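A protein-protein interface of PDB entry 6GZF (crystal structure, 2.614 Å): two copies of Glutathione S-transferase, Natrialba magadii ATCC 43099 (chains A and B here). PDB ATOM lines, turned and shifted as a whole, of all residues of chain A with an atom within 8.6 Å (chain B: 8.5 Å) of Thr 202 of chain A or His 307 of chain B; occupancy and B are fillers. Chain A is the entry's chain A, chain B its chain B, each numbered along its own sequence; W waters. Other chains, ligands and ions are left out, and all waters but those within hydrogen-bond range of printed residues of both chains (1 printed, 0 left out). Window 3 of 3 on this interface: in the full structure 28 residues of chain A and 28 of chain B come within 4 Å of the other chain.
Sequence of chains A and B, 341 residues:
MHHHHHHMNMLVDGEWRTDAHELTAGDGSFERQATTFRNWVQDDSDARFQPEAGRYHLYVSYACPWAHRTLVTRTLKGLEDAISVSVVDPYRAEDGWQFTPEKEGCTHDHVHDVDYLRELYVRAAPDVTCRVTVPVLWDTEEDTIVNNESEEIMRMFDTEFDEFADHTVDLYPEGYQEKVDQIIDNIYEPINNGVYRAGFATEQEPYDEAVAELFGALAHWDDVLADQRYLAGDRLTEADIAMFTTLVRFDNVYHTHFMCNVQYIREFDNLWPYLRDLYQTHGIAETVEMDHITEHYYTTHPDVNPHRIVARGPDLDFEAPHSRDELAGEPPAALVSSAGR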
ATOM      1  N   HIS A   3       0.394   5.407   3.651  1.00  0.00           N
ATOM      2  CA  HIS A   3      -0.172   6.438   4.519  1.00  0.00           C
ATOM      3  C   HIS A   3       0.312   7.842   4.151  1.00  0.00           C
ATOM      4  O   HIS A   3       1.503   8.065   3.930  1.00  0.00           O
ATOM      5  CB  HIS A   3       0.152   6.132   5.983  1.00  0.00           C
ATOM      6  CG  HIS A   3      -0.460   4.863   6.482  1.00  0.00           C
ATOM      7  ND1 HIS A   3      -1.697   4.822   7.103  1.00  0.00           N
ATOM      8  CD2 HIS A   3      -0.023   3.583   6.451  1.00  0.00           C
ATOM      9  CE1 HIS A   3      -1.984   3.580   7.429  1.00  0.00           C
ATOM     10  NE2 HIS A   3      -0.982   2.803   7.045  1.00  0.00           N
ATOM     11  N   HIS A   5      -0.220  12.358   4.614  1.00  0.00           N
ATOM     12  CA  HIS A   5      -0.571  13.403   5.575  1.00  0.00           C
ATOM     13  C   HIS A   5      -1.923  14.043   5.267  1.00  0.00           C
ATOM     14  O   HIS A   5      -2.336  14.128   4.111  1.00  0.00           O
ATOM     15  CB  HIS A   5       0.533  14.467   5.639  1.00  0.00           C
ATOM     16  CG  HIS A   5       0.467  15.494   4.550  1.00  0.00           C
ATOM     17  ND1 HIS A   5       1.015  15.293   3.300  1.00  0.00           N
ATOM     18  CD2 HIS A   5      -0.054  16.743   4.536  1.00  0.00           C
ATOM     19  CE1 HIS A   5       0.822  16.369   2.560  1.00  0.00           C
ATOM     20  NE2 HIS A   5       0.174  17.264   3.286  1.00  0.00           N
ATOM     21  N   HIS A   6      -2.595  14.494   6.324  1.00  0.00           N
ATOM     22  CA  HIS A   6      -4.004  14.889   6.275  1.00  0.00           C
ATOM     23  C   HIS A   6      -4.356  15.914   5.197  1.00  0.00           C
ATOM     24  O   HIS A   6      -5.513  16.014   4.788  1.00  0.00           O
ATOM     25  CB  HIS A   6      -4.431  15.437   7.639  1.00  0.00           C
ATOM     26  CG  HIS A   6      -4.344  14.437   8.750  1.00  0.00           C
ATOM     27  ND1 HIS A   6      -5.125  13.302   8.794  1.00  0.00           N
ATOM     28  CD2 HIS A   6      -3.572  14.405   9.862  1.00  0.00           C
ATOM     29  CE1 HIS A   6      -4.835  12.612   9.882  1.00  0.00           C
ATOM     30  NE2 HIS A   6      -3.896  13.260  10.549  1.00  0.00           N
ATOM     31  N   HIS A   7      -3.368  16.676   4.739  1.00  0.00           N
ATOM     32  CA  HIS A   7      -3.613  17.687   3.719  1.00  0.00           C
ATOM     33  C   HIS A   7      -2.939  17.345   2.395  1.00  0.00           C
ATOM     34  O   HIS A   7      -2.633  18.234   1.600  1.00  0.00           O
ATOM     35  CB  HIS A   7      -3.143  19.061   4.202  1.00  0.00           C
ATOM     36  CG  HIS A   7      -4.115  19.749   5.108  1.00  0.00           C
ATOM     37  ND1 HIS A   7      -5.003  20.702   4.658  1.00  0.00           N
ATOM     38  CD2 HIS A   7      -4.337  19.625   6.438  1.00  0.00           C
ATOM     39  CE1 HIS A   7      -5.732  21.135   5.672  1.00  0.00           C
ATOM     40  NE2 HIS A   7      -5.348  20.498   6.763  1.00  0.00           N
ATOM     41  N   ASP A  27     -10.631   3.718   4.828  1.00  0.00           N
ATOM     42  CA  ASP A  27      -9.174   3.636   4.961  1.00  0.00           C
ATOM     43  C   ASP A  27      -8.449   3.545   3.617  1.00  0.00           C
ATOM     44  O   ASP A  27      -8.493   2.510   2.951  1.00  0.00           O
ATOM     45  CB  ASP A  27      -8.798   2.431   5.829  1.00  0.00           C
ATOM     46  CG  ASP A  27      -9.083   2.663   7.295  1.00  0.00           C
ATOM     47  OD1 ASP A  27      -9.919   3.541   7.602  1.00  0.00           O
ATOM     48  OD2 ASP A  27      -8.467   1.967   8.132  1.00  0.00           O
ATOM     49  N   TYR A 196       3.967   6.010   9.981  1.00  0.00           N
ATOM     50  CA  TYR A 196       3.025   6.922   9.342  1.00  0.00           C
ATOM     51  C   TYR A 196       1.588   6.566   9.701  1.00  0.00           C
ATOM     52  O   TYR A 196       0.723   7.438   9.783  1.00  0.00           O
ATOM     53  CB  TYR A 196       3.207   6.911   7.822  1.00  0.00           C
ATOM     54  CG  TYR A 196       4.532   7.478   7.368  1.00  0.00           C
ATOM     55  CD1 TYR A 196       5.660   6.674   7.279  1.00  0.00           C
ATOM     56  CD2 TYR A 196       4.655   8.821   7.035  1.00  0.00           C
ATOM     57  CE1 TYR A 196       6.873   7.190   6.868  1.00  0.00           C
ATOM     58  CE2 TYR A 196       5.864   9.347   6.623  1.00  0.00           C
ATOM     59  CZ  TYR A 196       6.970   8.527   6.542  1.00  0.00           C
ATOM     60  OH  TYR A 196       8.173   9.049   6.132  1.00  0.00           O
ATOM     61  N   ARG A 197       1.340   5.278   9.915  1.00  0.00           N
ATOM     62  CA  ARG A 197       0.028   4.815  10.346  1.00  0.00           C
ATOM     63  C   ARG A 197      -0.263   5.332  11.748  1.00  0.00           C
ATOM     64  O   ARG A 197      -1.392   5.700  12.066  1.00  0.00           O
ATOM     65  CB  ARG A 197      -0.046   3.287  10.305  1.00  0.00           C
ATOM     66  CG  ARG A 197      -1.348   2.701  10.830  1.00  0.00           C
ATOM     67  CD  ARG A 197      -1.543   1.275  10.342  1.00  0.00           C
ATOM     68  NE  ARG A 197      -2.646   0.601  11.021  1.00  0.00           N
ATOM     69  CZ  ARG A 197      -2.488  -0.351  11.937  1.00  0.00           C
ATOM     70  NH1 ARG A 197      -3.548  -0.911  12.504  1.00  0.00           N
ATOM     71  NH2 ARG A 197      -1.271  -0.748  12.280  1.00  0.00           N
ATOM     72  N   ALA A 198       0.774   5.368  12.579  1.00  0.00           N
ATOM     73  CA  ALA A 198       0.655   5.889  13.933  1.00  0.00           C
ATOM     74  C   ALA A 198       0.546   7.411  13.925  1.00  0.00           C
ATOM     75  O   ALA A 198      -0.196   7.993  14.715  1.00  0.00           O
ATOM     76  CB  ALA A 198       1.841   5.447  14.775  1.00  0.00           C
ATOM     77  N   GLY A 199       1.287   8.048  13.023  1.00  0.00           N
ATOM     78  CA  GLY A 199       1.339   9.497  12.956  1.00  0.00           C
ATOM     79  C   GLY A 199       0.079  10.149  12.420  1.00  0.00           C
ATOM     80  O   GLY A 199      -0.390  11.148  12.966  1.00  0.00           O
ATOM     81  N   PHE A 200      -0.468   9.591  11.346  1.00  0.00           N
ATOM     82  CA  PHE A 200      -1.679  10.131  10.739  1.00  0.00           C
ATOM     83  C   PHE A 200      -2.925   9.438  11.279  1.00  0.00           C
ATOM     84  O   PHE A 200      -4.012   9.575  10.718  1.00  0.00           O
ATOM     85  CB  PHE A 200      -1.626   9.996   9.215  1.00  0.00           C
ATOM     86  CG  PHE A 200      -0.400  10.601   8.595  1.00  0.00           C
ATOM     87  CD1 PHE A 200       0.111  11.801   9.062  1.00  0.00           C
ATOM     88  CD2 PHE A 200       0.243   9.968   7.547  1.00  0.00           C
ATOM     89  CE1 PHE A 200       1.241  12.357   8.494  1.00  0.00           C
ATOM     90  CE2 PHE A 200       1.373  10.519   6.974  1.00  0.00           C
ATOM     91  CZ  PHE A 200       1.873  11.713   7.449  1.00  0.00           C
ATOM     92  N   ALA A 201      -2.758   8.694  12.370  1.00  0.00           N
ATOM     93  CA  ALA A 201      -3.875   8.006  13.010  1.00  0.00           C
ATOM     94  C   ALA A 201      -4.933   9.004  13.461  1.00  0.00           C
ATOM     95  O   ALA A 201      -4.614  10.035  14.052  1.00  0.00           O
ATOM     96  CB  ALA A 201      -3.387   7.182  14.190  1.00  0.00           C
ATOM     97  N   THR A 202      -6.193   8.696  13.174  1.00  0.00           N
ATOM     98  CA  THR A 202      -7.288   9.601  13.494  1.00  0.00           C
ATOM     99  C   THR A 202      -8.148   9.057  14.632  1.00  0.00           C
ATOM    100  O   THR A 202      -8.944   9.787  15.222  1.00  0.00           O
ATOM    101  CB  THR A 202      -8.175   9.864  12.260  1.00  0.00           C
ATOM    102  OG1 THR A 202      -8.973  11.034  12.480  1.00  0.00           O
ATOM    103  CG2 THR A 202      -9.077   8.671  11.974  1.00  0.00           C
ATOM    104  N   GLU A 203      -7.981   7.774  14.932  1.00  0.00           N
ATOM    105  CA  GLU A 203      -8.690   7.143  16.040  1.00  0.00           C
ATOM    106  C   GLU A 203      -7.691   6.464  16.972  1.00  0.00           C
ATOM    107  O   GLU A 203      -6.553   6.202  16.586  1.00  0.00           O
ATOM    108  CB  GLU A 203      -9.718   6.135  15.522  1.00  0.00           C
ATOM    109  CG  GLU A 203     -10.798   6.743  14.640  1.00  0.00           C
ATOM    110  CD  GLU A 203     -11.655   5.694  13.958  1.00  0.00           C
ATOM    111  OE1 GLU A 203     -11.091   4.697  13.461  1.00  0.00           O
ATOM    112  OE2 GLU A 203     -12.891   5.866  13.919  1.00  0.00           O
ATOM    113  N   GLN A 204      -8.118   6.180  18.198  1.00  0.00           N
ATOM    114  CA  GLN A 204      -7.211   5.655  19.215  1.00  0.00           C
ATOM    115  C   GLN A 204      -6.770   4.221  18.936  1.00  0.00           C
ATOM    116  O   GLN A 204      -5.578   3.913  18.988  1.00  0.00           O
ATOM    117  CB  GLN A 204      -7.860   5.732  20.597  1.00  0.00           C
ATOM    118  CG  GLN A 204      -6.915   5.378  21.734  1.00  0.00           C
ATOM    119  CD  GLN A 204      -5.716   6.306  21.803  1.00  0.00           C
ATOM    120  OE1 GLN A 204      -5.856   7.528  21.734  1.00  0.00           O
ATOM    121  NE2 GLN A 204      -4.527   5.727  21.935  1.00  0.00           N
ATOM    122  N   GLU A 205      -7.731   3.349  18.640  1.00  0.00           N
ATOM    123  CA  GLU A 205      -7.440   1.935  18.405  1.00  0.00           C
ATOM    124  C   GLU A 205      -6.458   1.687  17.243  1.00  0.00           C
ATOM    125  O   GLU A 205      -5.556   0.867  17.385  1.00  0.00           O
ATOM    126  CB  GLU A 205      -8.740   1.154  18.170  1.00  0.00           C
ATOM    127  CG  GLU A 205      -9.871   1.529  19.116  1.00  0.00           C
ATOM    128  CD  GLU A 205     -10.526   0.318  19.750  1.00  0.00           C
ATOM    129  OE1 GLU A 205     -11.689   0.017  19.403  1.00  0.00           O
ATOM    130  OE2 GLU A 205      -9.878  -0.330  20.599  1.00  0.00           O
ATOM    131  N   PRO A 206      -6.622   2.380  16.096  1.00  0.00           N
ATOM    132  CA  PRO A 206      -5.602   2.201  15.051  1.00  0.00           C
ATOM    133  C   PRO A 206      -4.206   2.641  15.490  1.00  0.00           C
ATOM    134  O   PRO A 206      -3.230   1.969  15.158  1.00  0.00           O
ATOM    135  CB  PRO A 206      -6.109   3.089  13.913  1.00  0.00           C
ATOM    136  CG  PRO A 206      -7.576   3.151  14.122  1.00  0.00           C
ATOM    137  CD  PRO A 206      -7.766   3.167  15.601  1.00  0.00           C
ATOM    138  N   TYR A 207      -4.118   3.750  16.221  1.00  0.00           N
ATOM    139  CA  TYR A 207      -2.839   4.223  16.742  1.00  0.00           C
ATOM    140  C   TYR A 207      -2.208   3.192  17.670  1.00  0.00           C
ATOM    141  O   TYR A 207      -1.014   2.910  17.578  1.00  0.00           O
ATOM    142  CB  TYR A 207      -3.015   5.554  17.480  1.00  0.00           C
ATOM    143  CG  TYR A 207      -1.807   5.978  18.291  1.00  0.00           C
ATOM    144  CD1 TYR A 207      -0.777   6.706  17.711  1.00  0.00           C
ATOM    145  CD2 TYR A 207      -1.702   5.658  19.641  1.00  0.00           C
ATOM    146  CE1 TYR A 207       0.327   7.097  18.448  1.00  0.00           C
ATOM    147  CE2 TYR A 207      -0.603   6.042  20.384  1.00  0.00           C
ATOM    148  CZ  TYR A 207       0.407   6.762  19.784  1.00  0.00           C
ATOM    149  OH  TYR A 207       1.502   7.146  20.524  1.00  0.00           O
ATOM    150  N   MET A 259       4.457  10.777  17.326  1.00  0.00           N
ATOM    151  CA  MET A 259       4.106  10.260  18.647  1.00  0.00           C
ATOM    152  C   MET A 259       4.397   8.769  18.825  1.00  0.00           C
ATOM    153  O   MET A 259       3.669   8.070  19.529  1.00  0.00           O
ATOM    154  CB  MET A 259       2.630  10.540  18.945  1.00  0.00           C
ATOM    155  CG  MET A 259       2.399  11.792  19.775  1.00  0.00           C
ATOM    156  SD  MET A 259       0.673  12.303  19.853  1.00  0.00           S
ATOM    157  CE  MET A 259       0.573  13.358  18.410  1.00  0.00           C
ATOM    158  N   PRO A 302       0.053  20.270   8.645  1.00  0.00           N
ATOM    159  CA  PRO A 302      -0.738  21.199   9.463  1.00  0.00           C
ATOM    160  C   PRO A 302      -1.636  20.506  10.488  1.00  0.00           C
ATOM    161  O   PRO A 302      -1.787  21.010  11.598  1.00  0.00           O
ATOM    162  CB  PRO A 302      -1.590  21.943   8.424  1.00  0.00           C
ATOM    163  CG  PRO A 302      -0.892  21.731   7.121  1.00  0.00           C
ATOM    164  CD  PRO A 302      -0.320  20.354   7.225  1.00  0.00           C
ATOM    165  N   ASP A 303      -2.227  19.373  10.121  1.00  0.00           N
ATOM    166  CA  ASP A 303      -3.165  18.690  11.007  1.00  0.00           C
ATOM    167  C   ASP A 303      -2.465  17.805  12.035  1.00  0.00           C
ATOM    168  O   ASP A 303      -3.117  17.181  12.872  1.00  0.00           O
ATOM    169  CB  ASP A 303      -4.156  17.855  10.197  1.00  0.00           C
ATOM    170  CG  ASP A 303      -5.397  18.636   9.809  1.00  0.00           C
ATOM    171  OD1 ASP A 303      -5.297  19.868   9.629  1.00  0.00           O
ATOM    172  OD2 ASP A 303      -6.476  18.016   9.687  1.00  0.00           O
ATOM    173  N   VAL A 304      -1.140  17.749  11.967  1.00  0.00           N
ATOM    174  CA  VAL A 304      -0.359  17.000  12.945  1.00  0.00           C
ATOM    175  C   VAL A 304       0.406  17.969  13.840  1.00  0.00           C
ATOM    176  O   VAL A 304       0.614  17.713  15.026  1.00  0.00           O
ATOM    177  CB  VAL A 304       0.625  16.029  12.267  1.00  0.00           C
ATOM    178  CG1 VAL A 304       1.262  15.110  13.299  1.00  0.00           C
ATOM    179  CG2 VAL A 304      -0.087  15.217  11.199  1.00  0.00           C
ATOM    180  N   ASN A 305       0.811  19.092  13.256  1.00  0.00           N
ATOM    181  CA  ASN A 305       1.565  20.114  13.971  1.00  0.00           C
ATOM    182  C   ASN A 305       1.223  21.505  13.439  1.00  0.00           C
ATOM    183  O   ASN A 305       1.974  22.069  12.644  1.00  0.00           O
ATOM    184  CB  ASN A 305       3.066  19.843  13.848  1.00  0.00           C
ATOM    185  CG  ASN A 305       3.899  20.742  14.737  1.00  0.00           C
ATOM    186  OD1 ASN A 305       3.538  21.009  15.883  1.00  0.00           O
ATOM    187  ND2 ASN A 305       5.023  21.212  14.212  1.00  0.00           N
ATOM    188  N   PRO A 306       0.080  22.057  13.883  1.00  0.00           N
ATOM    189  CA  PRO A 306      -0.522  23.297  13.372  1.00  0.00           C
ATOM    190  C   PRO A 306       0.421  24.497  13.292  1.00  0.00           C
ATOM    191  O   PRO A 306       0.414  25.203  12.283  1.00  0.00           O
ATOM    192  CB  PRO A 306      -1.642  23.573  14.379  1.00  0.00           C
ATOM    193  CG  PRO A 306      -2.025  22.230  14.874  1.00  0.00           C
ATOM    194  CD  PRO A 306      -0.739  21.456  14.950  1.00  0.00           C
ATOM    195  N   TYR B 298      -3.425  15.410  26.026  1.00  0.00           N
ATOM    196  CA  TYR B 298      -3.571  14.923  24.659  1.00  0.00           C
ATOM    197  C   TYR B 298      -4.978  15.119  24.094  1.00  0.00           C
ATOM    198  O   TYR B 298      -5.199  14.908  22.905  1.00  0.00           O
ATOM    199  CB  TYR B 298      -3.190  13.441  24.579  1.00  0.00           C
ATOM    200  CG  TYR B 298      -1.702  13.181  24.668  1.00  0.00           C
ATOM    201  CD1 TYR B 298      -0.855  13.533  23.626  1.00  0.00           C
ATOM    202  CD2 TYR B 298      -1.147  12.575  25.788  1.00  0.00           C
ATOM    203  CE1 TYR B 298       0.506  13.297  23.700  1.00  0.00           C
ATOM    204  CE2 TYR B 298       0.213  12.335  25.871  1.00  0.00           C
ATOM    205  CZ  TYR B 298       1.033  12.697  24.824  1.00  0.00           C
ATOM    206  OH  TYR B 298       2.386  12.458  24.903  1.00  0.00           O
ATOM    207  N   THR B 299      -5.924  15.530  24.934  1.00  0.00           N
ATOM    208  CA  THR B 299      -7.309  15.668  24.486  1.00  0.00           C
ATOM    209  C   THR B 299      -7.824  17.108  24.564  1.00  0.00           C
ATOM    210  O   THR B 299      -8.741  17.485  23.833  1.00  0.00           O
ATOM    211  CB  THR B 299      -8.254  14.760  25.307  1.00  0.00           C
ATOM    212  OG1 THR B 299      -7.640  13.480  25.507  1.00  0.00           O
ATOM    213  CG2 THR B 299      -9.588  14.574  24.597  1.00  0.00           C
ATOM    214  N   HIS B 301      -6.000  19.934  24.112  1.00  0.00           N
ATOM    215  CA  HIS B 301      -5.190  20.896  23.369  1.00  0.00           C
ATOM    216  C   HIS B 301      -5.335  20.708  21.858  1.00  0.00           C
ATOM    217  O   HIS B 301      -4.471  20.108  21.220  1.00  0.00           O
ATOM    218  CB  HIS B 301      -3.719  20.782  23.779  1.00  0.00           C
ATOM    219  CG  HIS B 301      -3.457  21.159  25.205  1.00  0.00           C
ATOM    220  ND1 HIS B 301      -2.262  20.894  25.838  1.00  0.00           N
ATOM    221  CD2 HIS B 301      -4.236  21.785  26.120  1.00  0.00           C
ATOM    222  CE1 HIS B 301      -2.316  21.337  27.081  1.00  0.00           C
ATOM    223  NE2 HIS B 301      -3.503  21.882  27.277  1.00  0.00           N
ATOM    224  N   PRO B 302      -6.431  21.233  21.284  1.00  0.00           N
ATOM    225  CA  PRO B 302      -6.767  21.075  19.863  1.00  0.00           C
ATOM    226  C   PRO B 302      -5.753  21.697  18.903  1.00  0.00           C
ATOM    227  O   PRO B 302      -5.660  21.254  17.759  1.00  0.00           O
ATOM    228  CB  PRO B 302      -8.118  21.790  19.742  1.00  0.00           C
ATOM    229  CG  PRO B 302      -8.680  21.784  21.123  1.00  0.00           C
ATOM    230  CD  PRO B 302      -7.491  21.949  22.014  1.00  0.00           C
ATOM    231  N   ASP B 303      -5.017  22.710  19.347  1.00  0.00           N
ATOM    232  CA  ASP B 303      -4.042  23.360  18.476  1.00  0.00           C
ATOM    233  C   ASP B 303      -2.634  22.818  18.697  1.00  0.00           C
ATOM    234  O   ASP B 303      -1.683  23.253  18.049  1.00  0.00           O
ATOM    235  CB  ASP B 303      -4.063  24.875  18.681  1.00  0.00           C
ATOM    236  CG  ASP B 303      -5.316  25.519  18.119  1.00  0.00           C
ATOM    237  OD1 ASP B 303      -6.073  24.826  17.406  1.00  0.00           O
ATOM    238  OD2 ASP B 303      -5.541  26.718  18.383  1.00  0.00           O
ATOM    239  N   VAL B 304      -2.510  21.868  19.616  1.00  0.00           N
ATOM    240  CA  VAL B 304      -1.245  21.179  19.839  1.00  0.00           C
ATOM    241  C   VAL B 304      -1.356  19.744  19.338  1.00  0.00           C
ATOM    242  O   VAL B 304      -0.414  19.195  18.767  1.00  0.00           O
ATOM    243  CB  VAL B 304      -0.847  21.181  21.328  1.00  0.00           C
ATOM    244  CG1 VAL B 304       0.547  20.596  21.507  1.00  0.00           C
ATOM    245  CG2 VAL B 304      -0.914  22.590  21.893  1.00  0.00           C
ATOM    246  N   ASN B 305      -2.525  19.149  19.552  1.00  0.00           N
ATOM    247  CA  ASN B 305      -2.795  17.783  19.122  1.00  0.00           C
ATOM    248  C   ASN B 305      -4.221  17.662  18.582  1.00  0.00           C
ATOM    249  O   ASN B 305      -5.113  17.184  19.284  1.00  0.00           O
ATOM    250  CB  ASN B 305      -2.575  16.811  20.281  1.00  0.00           C
ATOM    251  CG  ASN B 305      -2.595  15.362  19.842  1.00  0.00           C
ATOM    252  OD1 ASN B 305      -2.262  15.043  18.700  1.00  0.00           O
ATOM    253  ND2 ASN B 305      -2.986  14.475  20.750  1.00  0.00           N
ATOM    254  N   PRO B 306      -4.431  18.095  17.327  1.00  0.00           N
ATOM    255  CA  PRO B 306      -5.742  18.247  16.679  1.00  0.00           C
ATOM    256  C   PRO B 306      -6.669  17.037  16.790  1.00  0.00           C
ATOM    257  O   PRO B 306      -7.825  17.201  17.179  1.00  0.00           O
ATOM    258  CB  PRO B 306      -5.372  18.496  15.215  1.00  0.00           C
ATOM    259  CG  PRO B 306      -4.043  19.150  15.282  1.00  0.00           C
ATOM    260  CD  PRO B 306      -3.332  18.478  16.423  1.00  0.00           C
ATOM    261  N   HIS B 307      -6.177  15.850  16.454  1.00  0.00           N
ATOM    262  CA  HIS B 307      -7.025  14.662  16.438  1.00  0.00           C
ATOM    263  C   HIS B 307      -7.151  14.026  17.820  1.00  0.00           C
ATOM    264  O   HIS B 307      -7.776  12.976  17.974  1.00  0.00           O
ATOM    265  CB  HIS B 307      -6.493  13.646  15.427  1.00  0.00           C
ATOM    266  CG  HIS B 307      -6.633  14.089  14.004  1.00  0.00           C
ATOM    267  ND1 HIS B 307      -7.855  14.189  13.375  1.00  0.00           N
ATOM    268  CD2 HIS B 307      -5.709  14.470  13.091  1.00  0.00           C
ATOM    269  CE1 HIS B 307      -7.678  14.607  12.134  1.00  0.00           C
ATOM    270  NE2 HIS B 307      -6.384  14.785  11.937  1.00  0.00           N
ATOM    271  N   ARG B 308      -6.550  14.676  18.813  1.00  0.00           N
ATOM    272  CA  ARG B 308      -6.711  14.312  20.221  1.00  0.00           C
ATOM    273  C   ARG B 308      -6.396  12.846  20.524  1.00  0.00           C
ATOM    274  O   ARG B 308      -7.113  12.196  21.283  1.00  0.00           O
ATOM    275  CB  ARG B 308      -8.134  14.639  20.684  1.00  0.00           C
ATOM    276  CG  ARG B 308      -8.539  16.091  20.459  1.00  0.00           C
ATOM    277  CD  ARG B 308      -9.917  16.387  21.032  1.00  0.00           C
ATOM    278  NE  ARG B 308     -10.390  17.718  20.660  1.00  0.00           N
ATOM    279  CZ  ARG B 308     -10.982  18.565  21.496  1.00  0.00           C
ATOM    280  NH1 ARG B 308     -11.175  18.226  22.764  1.00  0.00           N
ATOM    281  NH2 ARG B 308     -11.380  19.755  21.066  1.00  0.00           N
ATOM    282  N   ILE B 309      -5.319  12.336  19.933  1.00  0.00           N
ATOM    283  CA  ILE B 309      -4.880  10.969  20.195  1.00  0.00           C
ATOM    284  C   ILE B 309      -3.901  10.929  21.364  1.00  0.00           C
ATOM    285  O   ILE B 309      -2.909  11.657  21.378  1.00  0.00           O
ATOM    286  CB  ILE B 309      -4.215  10.340  18.954  1.00  0.00           C
ATOM    287  CG1 ILE B 309      -5.206  10.278  17.791  1.00  0.00           C
ATOM    288  CG2 ILE B 309      -3.687   8.950  19.280  1.00  0.00           C
ATOM    289  CD1 ILE B 309      -6.466   9.501  18.110  1.00  0.00           C
ATOM    290  N   VAL B 310      -4.188  10.079  22.345  1.00  0.00           N
ATOM    291  CA  VAL B 310      -3.318   9.931  23.506  1.00  0.00           C
ATOM    292  C   VAL B 310      -2.125   9.036  23.187  1.00  0.00           C
ATOM    293  O   VAL B 310      -2.290   7.866  22.845  1.00  0.00           O
ATOM    294  CB  VAL B 310      -4.078   9.350  24.713  1.00  0.00           C
ATOM    295  CG1 VAL B 310      -3.119   9.065  25.858  1.00  0.00           C
ATOM    296  CG2 VAL B 310      -5.182  10.302  25.152  1.00  0.00           C
HETATM  297  O   HOH W   1     -10.413  11.881  17.035  1.00  0.00           O
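The side-chain amide nitrogen (ND2) of Asn 305 of chain B lies within hydrogen-bond range of the backbone carbonyl oxygen (O) of Tyr 298 of chain B.
O of Ile 309 of chain B is in hydrogen-bond range of ND2 of Asn 305 of chain B (2.9 Å).
The side-chain carboxylate (OD1) of Asp 303 of chain A is in hydrogen-bond range of a ring nitrogen (NE2) of His 7 of chain A.
The backbone carbonyl oxygen (O) of Met 259 of chain A is in hydrogen-bond range of the side-chain hydroxyl (OH) of Tyr 207 of chain A (2.6 Å).
Water W1 bridges O of His 307 of chain B (3.0 Å) and O of Thr 202 of chain A (3.1 Å).
The side-chain hydroxyl (OG1) of Thr 202 of chain A is in hydrogen-bond range of a ring nitrogen (ND1) of His 307 of chain B, at 3.5 Å.
OE1 of Gln 204 of chain A lies within hydrogen-bond range of N of Val 310 of chain B, at 3.1 Å.
A ring nitrogen (NE2) of His 307 of chain B lies within hydrogen-bond range of a ring nitrogen (NE2) of His 6 of chain A (3.2 Å).
Of chain A, only His 6, Thr 202 and Asp 303 come within 4 Å of His 307 of chain B.
Ala 201 of chain A touches one residue of chain B.
Pro 306 of chain B touches just these residues of chain A: Asp 303 and Pro 306.
Printed residues of chain A within 4 Å of Tyr 298 of chain B: Met 259.
Of the printed residues of chain B, Asp 303 of chain A touches Pro 306 (3.2 Å) and His 307 (3.8 Å).
Printed residues of chain B within 4 Å of Met 259 of chain A: Tyr 298 (3.98 Å), Asn 305 (3.3 Å) and Ile 309 (3.9 Å).
Of the printed residues of chain B, Glu 203 of chain A touches Ile 309.
The nearest residue of chain A that does not touch His 307 of chain B is Ala 201 of chain A (4.3 Å).
CG1 of Ile 309 of chain B touches O of Ala 201 of chain A, 3.8 Å away.
Thr 202 of chain A touches Ile 309 of chain B (O to CD1, 3.8 Å).
Ile 309 of chain B touches Gln 204 of chain A.
Ile 309 of chain B touches Tyr 207 of chain A (CG2 to CG, 3.7 Å).
Val 310 of chain B touches Tyr 207 of chain A (O to CE2, 3.5 Å).
SD of Met 259 of chain A touches CE1 of Tyr 298 of chain B, 3.98 Å away.
Met 259 of chain A touches Asn 305 of chain B (CE to OD1, 3.3 Å).
Met 259 of chain A touches Ile 309 of chain B.
His 307 of chain B touches Asp 303 of chain A.
Asp 303 of chain B touches Pro 306 of chain A.
Along chain B the printed residues that touch a printed residue of chain A span positions 298 to 310.
Among the printed residues, 16 pairs touch across the chains.
Asp 303 of chain A touches Pro 306 of chain B, and with the chains exchanged Pro 306 of chain A touches Asp 303 of chain B.
Pro 306 of chain B touches its own counterpart, Pro 306 of chain A.
Of the 16 pairs that touch across the chains among the printed residues, 3 have their exchanged pair printed and touching as well.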
